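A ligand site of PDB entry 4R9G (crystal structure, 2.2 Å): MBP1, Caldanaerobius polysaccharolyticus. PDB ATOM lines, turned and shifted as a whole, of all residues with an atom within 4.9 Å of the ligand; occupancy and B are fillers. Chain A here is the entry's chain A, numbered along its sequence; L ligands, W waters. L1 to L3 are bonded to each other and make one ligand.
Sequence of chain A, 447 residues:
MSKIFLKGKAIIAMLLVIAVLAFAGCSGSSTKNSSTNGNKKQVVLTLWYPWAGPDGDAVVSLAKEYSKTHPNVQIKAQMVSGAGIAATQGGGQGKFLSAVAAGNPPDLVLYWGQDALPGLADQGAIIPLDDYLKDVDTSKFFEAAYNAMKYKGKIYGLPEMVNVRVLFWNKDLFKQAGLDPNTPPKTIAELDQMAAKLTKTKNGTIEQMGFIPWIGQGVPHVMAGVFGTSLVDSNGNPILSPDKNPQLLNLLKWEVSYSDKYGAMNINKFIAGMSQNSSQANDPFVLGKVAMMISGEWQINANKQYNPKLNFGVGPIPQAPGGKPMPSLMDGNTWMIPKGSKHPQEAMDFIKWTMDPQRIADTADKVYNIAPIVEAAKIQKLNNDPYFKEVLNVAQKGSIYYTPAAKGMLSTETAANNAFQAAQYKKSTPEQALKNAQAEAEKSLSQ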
ATOM      1  N   TRP A  51       3.723 -14.876 -24.199  1.00  0.00           N
ATOM      2  CA  TRP A  51       2.564 -14.918 -25.119  1.00  0.00           C
ATOM      3  C   TRP A  51       2.962 -14.599 -26.566  1.00  0.00           C
ATOM      4  O   TRP A  51       4.014 -13.961 -26.804  1.00  0.00           O
ATOM      5  CB  TRP A  51       1.381 -14.018 -24.683  1.00  0.00           C
ATOM      6  CG  TRP A  51       1.715 -12.805 -23.808  1.00  0.00           C
ATOM      7  CD1 TRP A  51       1.032 -12.402 -22.685  1.00  0.00           C
ATOM      8  CD2 TRP A  51       2.775 -11.847 -23.999  1.00  0.00           C
ATOM      9  NE1 TRP A  51       1.607 -11.273 -22.155  1.00  0.00           N
ATOM     10  CE2 TRP A  51       2.680 -10.907 -22.938  1.00  0.00           C
ATOM     11  CE3 TRP A  51       3.800 -11.707 -24.948  1.00  0.00           C
ATOM     12  CZ2 TRP A  51       3.564  -9.828 -22.797  1.00  0.00           C
ATOM     13  CZ3 TRP A  51       4.714 -10.628 -24.808  1.00  0.00           C
ATOM     14  CH2 TRP A  51       4.572  -9.702 -23.736  1.00  0.00           C
ATOM     15  N   ASP A  55       1.681  -8.751 -28.672  1.00  0.00           N
ATOM     16  CA  ASP A  55       2.662  -8.529 -27.602  1.00  0.00           C
ATOM     17  C   ASP A  55       3.899  -9.339 -27.885  1.00  0.00           C
ATOM     18  O   ASP A  55       4.993  -8.875 -27.629  1.00  0.00           O
ATOM     19  CB  ASP A  55       2.129  -8.921 -26.221  1.00  0.00           C
ATOM     20  CG  ASP A  55       0.961  -8.085 -25.803  1.00  0.00           C
ATOM     21  OD1 ASP A  55       1.099  -7.343 -24.815  1.00  0.00           O
ATOM     22  OD2 ASP A  55      -0.097  -8.188 -26.443  1.00  0.00           O
ATOM     23  N   ALA A  86       3.610 -19.698 -14.680  1.00  0.00           N
ATOM     24  CA  ALA A  86       2.256 -19.369 -14.190  1.00  0.00           C
ATOM     25  C   ALA A  86       1.463 -20.550 -13.625  1.00  0.00           C
ATOM     26  O   ALA A  86       1.377 -21.624 -14.265  1.00  0.00           O
ATOM     27  CB  ALA A  86       1.454 -18.659 -15.279  1.00  0.00           C
ATOM     28  N   TRP A 112       4.033 -12.428 -17.043  1.00  0.00           N
ATOM     29  CA  TRP A 112       2.850 -11.618 -17.324  1.00  0.00           C
ATOM     30  C   TRP A 112       2.126 -11.099 -16.086  1.00  0.00           C
ATOM     31  O   TRP A 112       0.974 -10.634 -16.174  1.00  0.00           O
ATOM     32  CB  TRP A 112       1.886 -12.345 -18.255  1.00  0.00           C
ATOM     33  CG  TRP A 112       1.332 -13.650 -17.740  1.00  0.00           C
ATOM     34  CD1 TRP A 112       1.033 -13.979 -16.433  1.00  0.00           C
ATOM     35  CD2 TRP A 112       0.950 -14.794 -18.531  1.00  0.00           C
ATOM     36  NE1 TRP A 112       0.504 -15.243 -16.370  1.00  0.00           N
ATOM     37  CE2 TRP A 112       0.445 -15.773 -17.639  1.00  0.00           C
ATOM     38  CE3 TRP A 112       0.982 -15.077 -19.901  1.00  0.00           C
ATOM     39  CZ2 TRP A 112      -0.015 -17.022 -18.073  1.00  0.00           C
ATOM     40  CZ3 TRP A 112       0.522 -16.326 -20.335  1.00  0.00           C
ATOM     41  CH2 TRP A 112       0.037 -17.283 -19.421  1.00  0.00           C
ATOM     42  N   MET A 161       5.578  -3.385 -17.977  1.00  0.00           N
ATOM     43  CA  MET A 161       4.343  -2.665 -18.346  1.00  0.00           C
ATOM     44  C   MET A 161       3.444  -2.599 -17.102  1.00  0.00           C
ATOM     45  O   MET A 161       3.611  -3.398 -16.190  1.00  0.00           O
ATOM     46  CB  MET A 161       3.582  -3.412 -19.436  1.00  0.00           C
ATOM     47  CG  MET A 161       4.098  -3.190 -20.858  1.00  0.00           C
ATOM     48  SD  MET A 161       4.015  -1.485 -21.440  1.00  0.00           S
ATOM     49  CE  MET A 161       5.470  -1.501 -22.498  1.00  0.00           C
ATOM     50  N   ASN A 163      -0.635  -2.808 -15.850  1.00  0.00           N
ATOM     51  CA  ASN A 163      -1.950  -3.223 -16.291  1.00  0.00           C
ATOM     52  C   ASN A 163      -3.061  -2.975 -15.281  1.00  0.00           C
ATOM     53  O   ASN A 163      -2.837  -2.989 -14.066  1.00  0.00           O
ATOM     54  CB  ASN A 163      -1.920  -4.698 -16.694  1.00  0.00           C
ATOM     55  CG  ASN A 163      -1.075  -4.940 -17.945  1.00  0.00           C
ATOM     56  OD1 ASN A 163      -0.263  -5.843 -17.986  1.00  0.00           O
ATOM     57  ND2 ASN A 163      -1.252  -4.098 -18.950  1.00  0.00           N
ATOM     58  N   ARG A 165      -7.533  -3.825 -14.529  1.00  0.00           N
ATOM     59  CA  ARG A 165      -8.662  -4.680 -14.884  1.00  0.00           C
ATOM     60  C   ARG A 165      -9.895  -3.798 -15.049  1.00  0.00           C
ATOM     61  O   ARG A 165     -10.125  -2.873 -14.268  1.00  0.00           O
ATOM     62  CB  ARG A 165      -8.883  -5.735 -13.833  1.00  0.00           C
ATOM     63  CG  ARG A 165      -7.692  -6.658 -13.603  1.00  0.00           C
ATOM     64  CD  ARG A 165      -7.182  -7.261 -14.907  1.00  0.00           C
ATOM     65  NE  ARG A 165      -6.245  -8.338 -14.701  1.00  0.00           N
ATOM     66  CZ  ARG A 165      -4.939  -8.197 -14.486  1.00  0.00           C
ATOM     67  NH1 ARG A 165      -4.364  -7.006 -14.435  1.00  0.00           N
ATOM     68  NH2 ARG A 165      -4.190  -9.274 -14.319  1.00  0.00           N
ATOM     69  N   GLN A 217     -10.718 -11.948 -17.505  1.00  0.00           N
ATOM     70  CA  GLN A 217      -9.923 -11.788 -16.322  1.00  0.00           C
ATOM     71  C   GLN A 217     -10.779 -12.046 -15.097  1.00  0.00           C
ATOM     72  O   GLN A 217     -10.393 -11.704 -14.004  1.00  0.00           O
ATOM     73  CB  GLN A 217      -9.270 -10.404 -16.305  1.00  0.00           C
ATOM     74  CG  GLN A 217      -8.194 -10.286 -17.373  1.00  0.00           C
ATOM     75  CD  GLN A 217      -6.925 -11.019 -16.935  1.00  0.00           C
ATOM     76  OE1 GLN A 217      -6.444 -10.781 -15.834  1.00  0.00           O
ATOM     77  NE2 GLN A 217      -6.390 -11.901 -17.794  1.00  0.00           N
ATOM     78  N   VAL A 219     -11.012 -14.283 -13.097  1.00  0.00           N
ATOM     79  CA  VAL A 219     -10.388 -15.433 -12.423  1.00  0.00           C
ATOM     80  C   VAL A 219     -10.214 -15.159 -10.907  1.00  0.00           C
ATOM     81  O   VAL A 219     -10.146 -13.990 -10.520  1.00  0.00           O
ATOM     82  CB  VAL A 219      -9.053 -15.792 -13.118  1.00  0.00           C
ATOM     83  CG1 VAL A 219      -9.326 -16.396 -14.488  1.00  0.00           C
ATOM     84  CG2 VAL A 219      -8.165 -14.546 -13.289  1.00  0.00           C
ATOM     85  N   HIS A 221      -7.908 -15.073  -8.524  1.00  0.00           N
ATOM     86  CA  HIS A 221      -6.871 -14.125  -8.074  1.00  0.00           C
ATOM     87  C   HIS A 221      -7.145 -12.643  -8.441  1.00  0.00           C
ATOM     88  O   HIS A 221      -6.574 -11.755  -7.806  1.00  0.00           O
ATOM     89  CB  HIS A 221      -5.428 -14.588  -8.440  1.00  0.00           C
ATOM     90  CG  HIS A 221      -5.075 -14.426  -9.886  1.00  0.00           C
ATOM     91  ND1 HIS A 221      -3.775 -14.225 -10.315  1.00  0.00           N
ATOM     92  CD2 HIS A 221      -5.835 -14.431 -11.006  1.00  0.00           C
ATOM     93  CE1 HIS A 221      -3.757 -14.104 -11.627  1.00  0.00           C
ATOM     94  NE2 HIS A 221      -4.993 -14.222 -12.078  1.00  0.00           N
ATOM     95  N   ASN A 277      -9.470 -17.648 -20.774  1.00  0.00           N
ATOM     96  CA  ASN A 277      -8.734 -16.733 -19.919  1.00  0.00           C
ATOM     97  C   ASN A 277      -7.470 -16.117 -20.531  1.00  0.00           C
ATOM     98  O   ASN A 277      -6.654 -15.522 -19.825  1.00  0.00           O
ATOM     99  CB  ASN A 277      -8.498 -17.337 -18.530  1.00  0.00           C
ATOM    100  CG  ASN A 277      -9.784 -17.803 -17.884  1.00  0.00           C
ATOM    101  OD1 ASN A 277      -9.956 -18.983 -17.687  1.00  0.00           O
ATOM    102  ND2 ASN A 277     -10.722 -16.892 -17.612  1.00  0.00           N
ATOM    103  N   SER A 278      -7.323 -16.287 -21.843  1.00  0.00           N
ATOM    104  CA  SER A 278      -6.332 -15.552 -22.624  1.00  0.00           C
ATOM    105  C   SER A 278      -7.100 -14.831 -23.706  1.00  0.00           C
ATOM    106  O   SER A 278      -8.061 -15.351 -24.273  1.00  0.00           O
ATOM    107  CB  SER A 278      -5.241 -16.460 -23.208  1.00  0.00           C
ATOM    108  OG  SER A 278      -5.813 -17.656 -23.716  1.00  0.00           O
ATOM    109  N   SER A 279      -6.716 -13.596 -23.949  1.00  0.00           N
ATOM    110  CA  SER A 279      -7.602 -12.699 -24.674  1.00  0.00           C
ATOM    111  C   SER A 279      -7.055 -12.514 -26.054  1.00  0.00           C
ATOM    112  O   SER A 279      -6.050 -11.850 -26.272  1.00  0.00           O
ATOM    113  CB  SER A 279      -7.836 -11.380 -23.917  1.00  0.00           C
ATOM    114  OG  SER A 279      -8.958 -11.519 -23.044  1.00  0.00           O
ATOM    115  N   TRP A 298      -5.497  -4.222 -22.145  1.00  0.00           N
ATOM    116  CA  TRP A 298      -4.982  -4.737 -23.430  1.00  0.00           C
ATOM    117  C   TRP A 298      -6.076  -5.240 -24.407  1.00  0.00           C
ATOM    118  O   TRP A 298      -5.901  -5.169 -25.620  1.00  0.00           O
ATOM    119  CB  TRP A 298      -3.977  -5.856 -23.179  1.00  0.00           C
ATOM    120  CG  TRP A 298      -4.547  -7.035 -22.410  1.00  0.00           C
ATOM    121  CD1 TRP A 298      -5.278  -8.072 -22.931  1.00  0.00           C
ATOM    122  CD2 TRP A 298      -4.418  -7.288 -21.000  1.00  0.00           C
ATOM    123  NE1 TRP A 298      -5.620  -8.963 -21.926  1.00  0.00           N
ATOM    124  CE2 TRP A 298      -5.099  -8.509 -20.737  1.00  0.00           C
ATOM    125  CE3 TRP A 298      -3.810  -6.610 -19.938  1.00  0.00           C
ATOM    126  CZ2 TRP A 298      -5.189  -9.078 -19.442  1.00  0.00           C
ATOM    127  CZ3 TRP A 298      -3.878  -7.173 -18.649  1.00  0.00           C
ATOM    128  CH2 TRP A 298      -4.573  -8.395 -18.412  1.00  0.00           C
ATOM    129  N   ASP A 331      -1.520  -4.270 -11.781  1.00  0.00           N
ATOM    130  CA  ASP A 331      -0.340  -5.111 -11.711  1.00  0.00           C
ATOM    131  C   ASP A 331       0.563  -4.800 -12.893  1.00  0.00           C
ATOM    132  O   ASP A 331       0.608  -3.654 -13.361  1.00  0.00           O
ATOM    133  CB  ASP A 331      -0.722  -6.602 -11.663  1.00  0.00           C
ATOM    134  CG  ASP A 331      -1.309  -7.110 -12.988  1.00  0.00           C
ATOM    135  OD1 ASP A 331      -1.703  -6.277 -13.852  1.00  0.00           O
ATOM    136  OD2 ASP A 331      -1.364  -8.348 -13.152  1.00  0.00           O
ATOM    137  N   ASN A 333       3.661  -6.630 -16.049  1.00  0.00           N
ATOM    138  CA  ASN A 333       4.607  -7.621 -16.524  1.00  0.00           C
ATOM    139  C   ASN A 333       5.918  -7.349 -15.811  1.00  0.00           C
ATOM    140  O   ASN A 333       6.225  -6.211 -15.491  1.00  0.00           O
ATOM    141  CB  ASN A 333       4.804  -7.474 -18.037  1.00  0.00           C
ATOM    142  CG  ASN A 333       3.529  -7.727 -18.810  1.00  0.00           C
ATOM    143  OD1 ASN A 333       2.649  -8.448 -18.349  1.00  0.00           O
ATOM    144  ND2 ASN A 333       3.422  -7.158 -20.004  1.00  0.00           N
ATOM    145  N   VAL A 367       1.010  -2.314 -27.774  1.00  0.00           N
ATOM    146  CA  VAL A 367       0.344  -3.429 -27.090  1.00  0.00           C
ATOM    147  C   VAL A 367      -0.853  -2.971 -26.248  1.00  0.00           C
ATOM    148  O   VAL A 367      -1.554  -3.799 -25.685  1.00  0.00           O
ATOM    149  CB  VAL A 367       1.322  -4.308 -26.252  1.00  0.00           C
ATOM    150  CG1 VAL A 367       2.549  -4.751 -27.077  1.00  0.00           C
ATOM    151  CG2 VAL A 367       1.794  -3.589 -24.995  1.00  0.00           C
ATOM    152  N   ASN A 369      -0.700  -1.156 -23.339  1.00  0.00           N
ATOM    153  CA  ASN A 369      -0.479  -1.278 -21.928  1.00  0.00           C
ATOM    154  C   ASN A 369      -0.187   0.103 -21.359  1.00  0.00           C
ATOM    155  O   ASN A 369      -0.089   1.089 -22.121  1.00  0.00           O
ATOM    156  CB  ASN A 369       0.668  -2.241 -21.678  1.00  0.00           C
ATOM    157  CG  ASN A 369       0.278  -3.706 -21.826  1.00  0.00           C
ATOM    158  OD1 ASN A 369       1.104  -4.558 -21.572  1.00  0.00           O
ATOM    159  ND2 ASN A 369      -0.956  -3.993 -22.225  1.00  0.00           N
ATOM    160  N   GLU A 413      -3.373 -20.401  -5.470  1.00  0.00           N
ATOM    161  CA  GLU A 413      -4.185 -20.089  -6.638  1.00  0.00           C
ATOM    162  C   GLU A 413      -4.689 -21.336  -7.338  1.00  0.00           C
ATOM    163  O   GLU A 413      -5.856 -21.377  -7.725  1.00  0.00           O
ATOM    164  CB  GLU A 413      -3.426 -19.246  -7.625  1.00  0.00           C
ATOM    165  CG  GLU A 413      -3.507 -17.760  -7.340  1.00  0.00           C
ATOM    166  CD  GLU A 413      -2.629 -16.962  -8.253  1.00  0.00           C
ATOM    167  OE1 GLU A 413      -2.413 -17.380  -9.423  1.00  0.00           O
ATOM    168  OE2 GLU A 413      -2.166 -15.898  -7.794  1.00  0.00           O
ATOM    169  N   ASN A 417      -8.408 -22.084  -8.049  1.00  0.00           N
ATOM    170  CA  ASN A 417      -8.943 -22.285  -9.397  1.00  0.00           C
ATOM    171  C   ASN A 417      -9.704 -23.596  -9.516  1.00  0.00           C
ATOM    172  O   ASN A 417     -10.782 -23.655 -10.109  1.00  0.00           O
ATOM    173  CB  ASN A 417      -7.838 -22.230 -10.458  1.00  0.00           C
ATOM    174  CG  ASN A 417      -7.173 -20.859 -10.554  1.00  0.00           C
ATOM    175  OD1 ASN A 417      -7.726 -19.834 -10.127  1.00  0.00           O
ATOM    176  ND2 ASN A 417      -5.996 -20.835 -11.144  1.00  0.00           N
HETATM  177  C1  LIG L   1      -5.129 -18.156 -14.781  1.00  0.00           C
HETATM  178  C2  LIG L   1      -4.233 -16.999 -14.353  1.00  0.00           C
HETATM  179  C3  LIG L   1      -4.115 -15.938 -15.461  1.00  0.00           C
HETATM  180  C4  LIG L   1      -3.993 -16.507 -16.879  1.00  0.00           C
HETATM  181  C5  LIG L   1      -4.894 -17.730 -17.047  1.00  0.00           C
HETATM  182  C6  LIG L   1      -4.689 -18.444 -18.372  1.00  0.00           C
HETATM  183  O1  LIG L   1      -6.431 -17.648 -14.964  1.00  0.00           O
HETATM  184  O2  LIG L   1      -2.952 -17.526 -14.085  1.00  0.00           O
HETATM  185  O3  LIG L   1      -2.972 -15.174 -15.162  1.00  0.00           O
HETATM  186  O4  LIG L   1      -4.386 -15.562 -17.854  1.00  0.00           O
HETATM  187  O5  LIG L   1      -4.659 -18.645 -16.001  1.00  0.00           O
HETATM  188  O6  LIG L   1      -3.321 -18.424 -18.636  1.00  0.00           O
HETATM  189  C1  LG2 L   2      -3.332 -14.629 -18.192  1.00  0.00           C
HETATM  190  C2  LG2 L   2      -3.394 -14.292 -19.673  1.00  0.00           C
HETATM  191  C3  LG2 L   2      -2.324 -13.229 -20.003  1.00  0.00           C
HETATM  192  C4  LG2 L   2      -2.446 -11.987 -19.131  1.00  0.00           C
HETATM  193  C5  LG2 L   2      -2.425 -12.435 -17.662  1.00  0.00           C
HETATM  194  C6  LG2 L   2      -2.643 -11.242 -16.741  1.00  0.00           C
HETATM  195  O1  LG2 L   2      -4.698 -13.798 -19.972  1.00  0.00           O
HETATM  196  O2  LG2 L   2      -2.307 -12.915 -21.407  1.00  0.00           O
HETATM  197  O3  LG2 L   2      -1.300 -11.152 -19.301  1.00  0.00           O
HETATM  198  O4  LG2 L   2      -3.418 -13.421 -17.408  1.00  0.00           O
HETATM  199  O5  LG2 L   2      -2.379 -11.609 -15.383  1.00  0.00           O
HETATM  200  C1  LG3 L   3      -1.565  -9.979 -20.052  1.00  0.00           C
HETATM  201  C2  LG3 L   3      -0.474  -8.951 -19.752  1.00  0.00           C
HETATM  202  C3  LG3 L   3      -0.542  -7.740 -20.670  1.00  0.00           C
HETATM  203  C4  LG3 L   3      -0.609  -8.205 -22.125  1.00  0.00           C
HETATM  204  C5  LG3 L   3      -1.676  -9.265 -22.365  1.00  0.00           C
HETATM  205  C6  LG3 L   3      -1.516  -9.866 -23.771  1.00  0.00           C
HETATM  206  O1  LG3 L   3       0.819  -9.543 -19.918  1.00  0.00           O
HETATM  207  O2  LG3 L   3       0.627  -6.938 -20.483  1.00  0.00           O
HETATM  208  O3  LG3 L   3      -0.877  -7.085 -22.971  1.00  0.00           O
HETATM  209  O4  LG3 L   3      -1.551 -10.340 -21.426  1.00  0.00           O
HETATM  210  O5  LG3 L   3      -2.600 -10.765 -23.923  1.00  0.00           O
HETATM  211  O   HOH W   1      -1.009 -16.106 -13.902  1.00  0.00           O
HETATM  212  O   HOH W   2      -4.569 -12.442 -22.776  1.00  0.00           O
HETATM  213  O   HOH W   3      -7.418 -18.025 -12.497  1.00  0.00           O
HETATM  214  O   HOH W   4       2.780  -6.282 -22.910  1.00  0.00           O
HETATM  215  O   HOH W   5      -0.672 -13.690 -13.219  1.00  0.00           O
HETATM  216  O   HOH W   6      -2.083 -19.795 -17.082  1.00  0.00           O
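The backbone NH (N) of Asn 333 is in hydrogen-bond range of the backbone carbonyl oxygen (O) of Met 161. The side-chain amide nitrogen of Asn 369 sits close to the side-chain amide nitrogen of Asn 163, 3.3 Å away. N of Asn 163 lies within hydrogen-bond range of O of Asp 331, 2.9 Å away. OE1 of Gln 217 sits at hydrogen-bond distance from NE of Arg 165 (2.7 Å). NH1 of Arg 165 is in salt-bridge range of OD1 of Asp 331, at 2.8 Å.
O of Asn 277 is in hydrogen-bond range of O1 of LG2 L2, 2.6 Å away. OD1 of Asn 333 sits at hydrogen-bond distance from O1 of LG3 L3 (2.6 Å). The side-chain amide oxygen (OD1) of Asn 369 is in hydrogen-bond range of an oxygen (O2) of LG3 L3 (2.7 Å). The side-chain carboxylate (OD1) of Asp 55 is in hydrogen-bond range of an oxygen (O3) of LG3 L3, at 2.7 Å. O2 of LG3 L3 lies within hydrogen-bond range of OD1 of Asn 163 (2.9 Å). An oxygen (O1) of LG3 L3 sits at hydrogen-bond distance from the indole nitrogen of Trp 51, at 2.9 Å. An oxygen (O5) of LG2 L2 lies within hydrogen-bond range of the guanidinium group (NH2) of Arg 165 (3.1 Å). The side-chain amide nitrogen (NE2) of Gln 217 is in hydrogen-bond range of an oxygen (O1) of LG2 L2 (3.3 Å).
Water W1 bridges an oxygen (O2) of LIG L1 (2.4 Å) and the indole nitrogen (NE1) of Trp 112 (3.0 Å). Water W3 lies within hydrogen-bond range of an oxygen (O1) of LIG L1 (2.7 Å) and the side-chain amide oxygen (OD1) of Asn 417 (3.0 Å). Water W2 lies within hydrogen-bond range of O2 of LG2 L2 (2.7 Å) and N of Ser 279 (2.7 Å). Water W4 lies within hydrogen-bond range of the side-chain amide oxygen (OD1) of Asn 369 (2.8 Å), the side-chain carboxylate (OD1) of Asp 55 (2.8 Å), the side-chain amide nitrogen (ND2) of Asn 333 (3.1 Å) and an oxygen (O2) of LG3 L3 (3.3 Å).
Residues that only touch the ligand: Val 219 (3.2 Å), Trp 298 (3.3 Å), Trp 112 (3.4 Å), Ser 278 (3.6 Å) and His 221 (3.7 Å). Hydrophobic or aromatic side chains that line the ligand: Trp 51, Trp 112, Val 219, His 221 and Trp 298.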
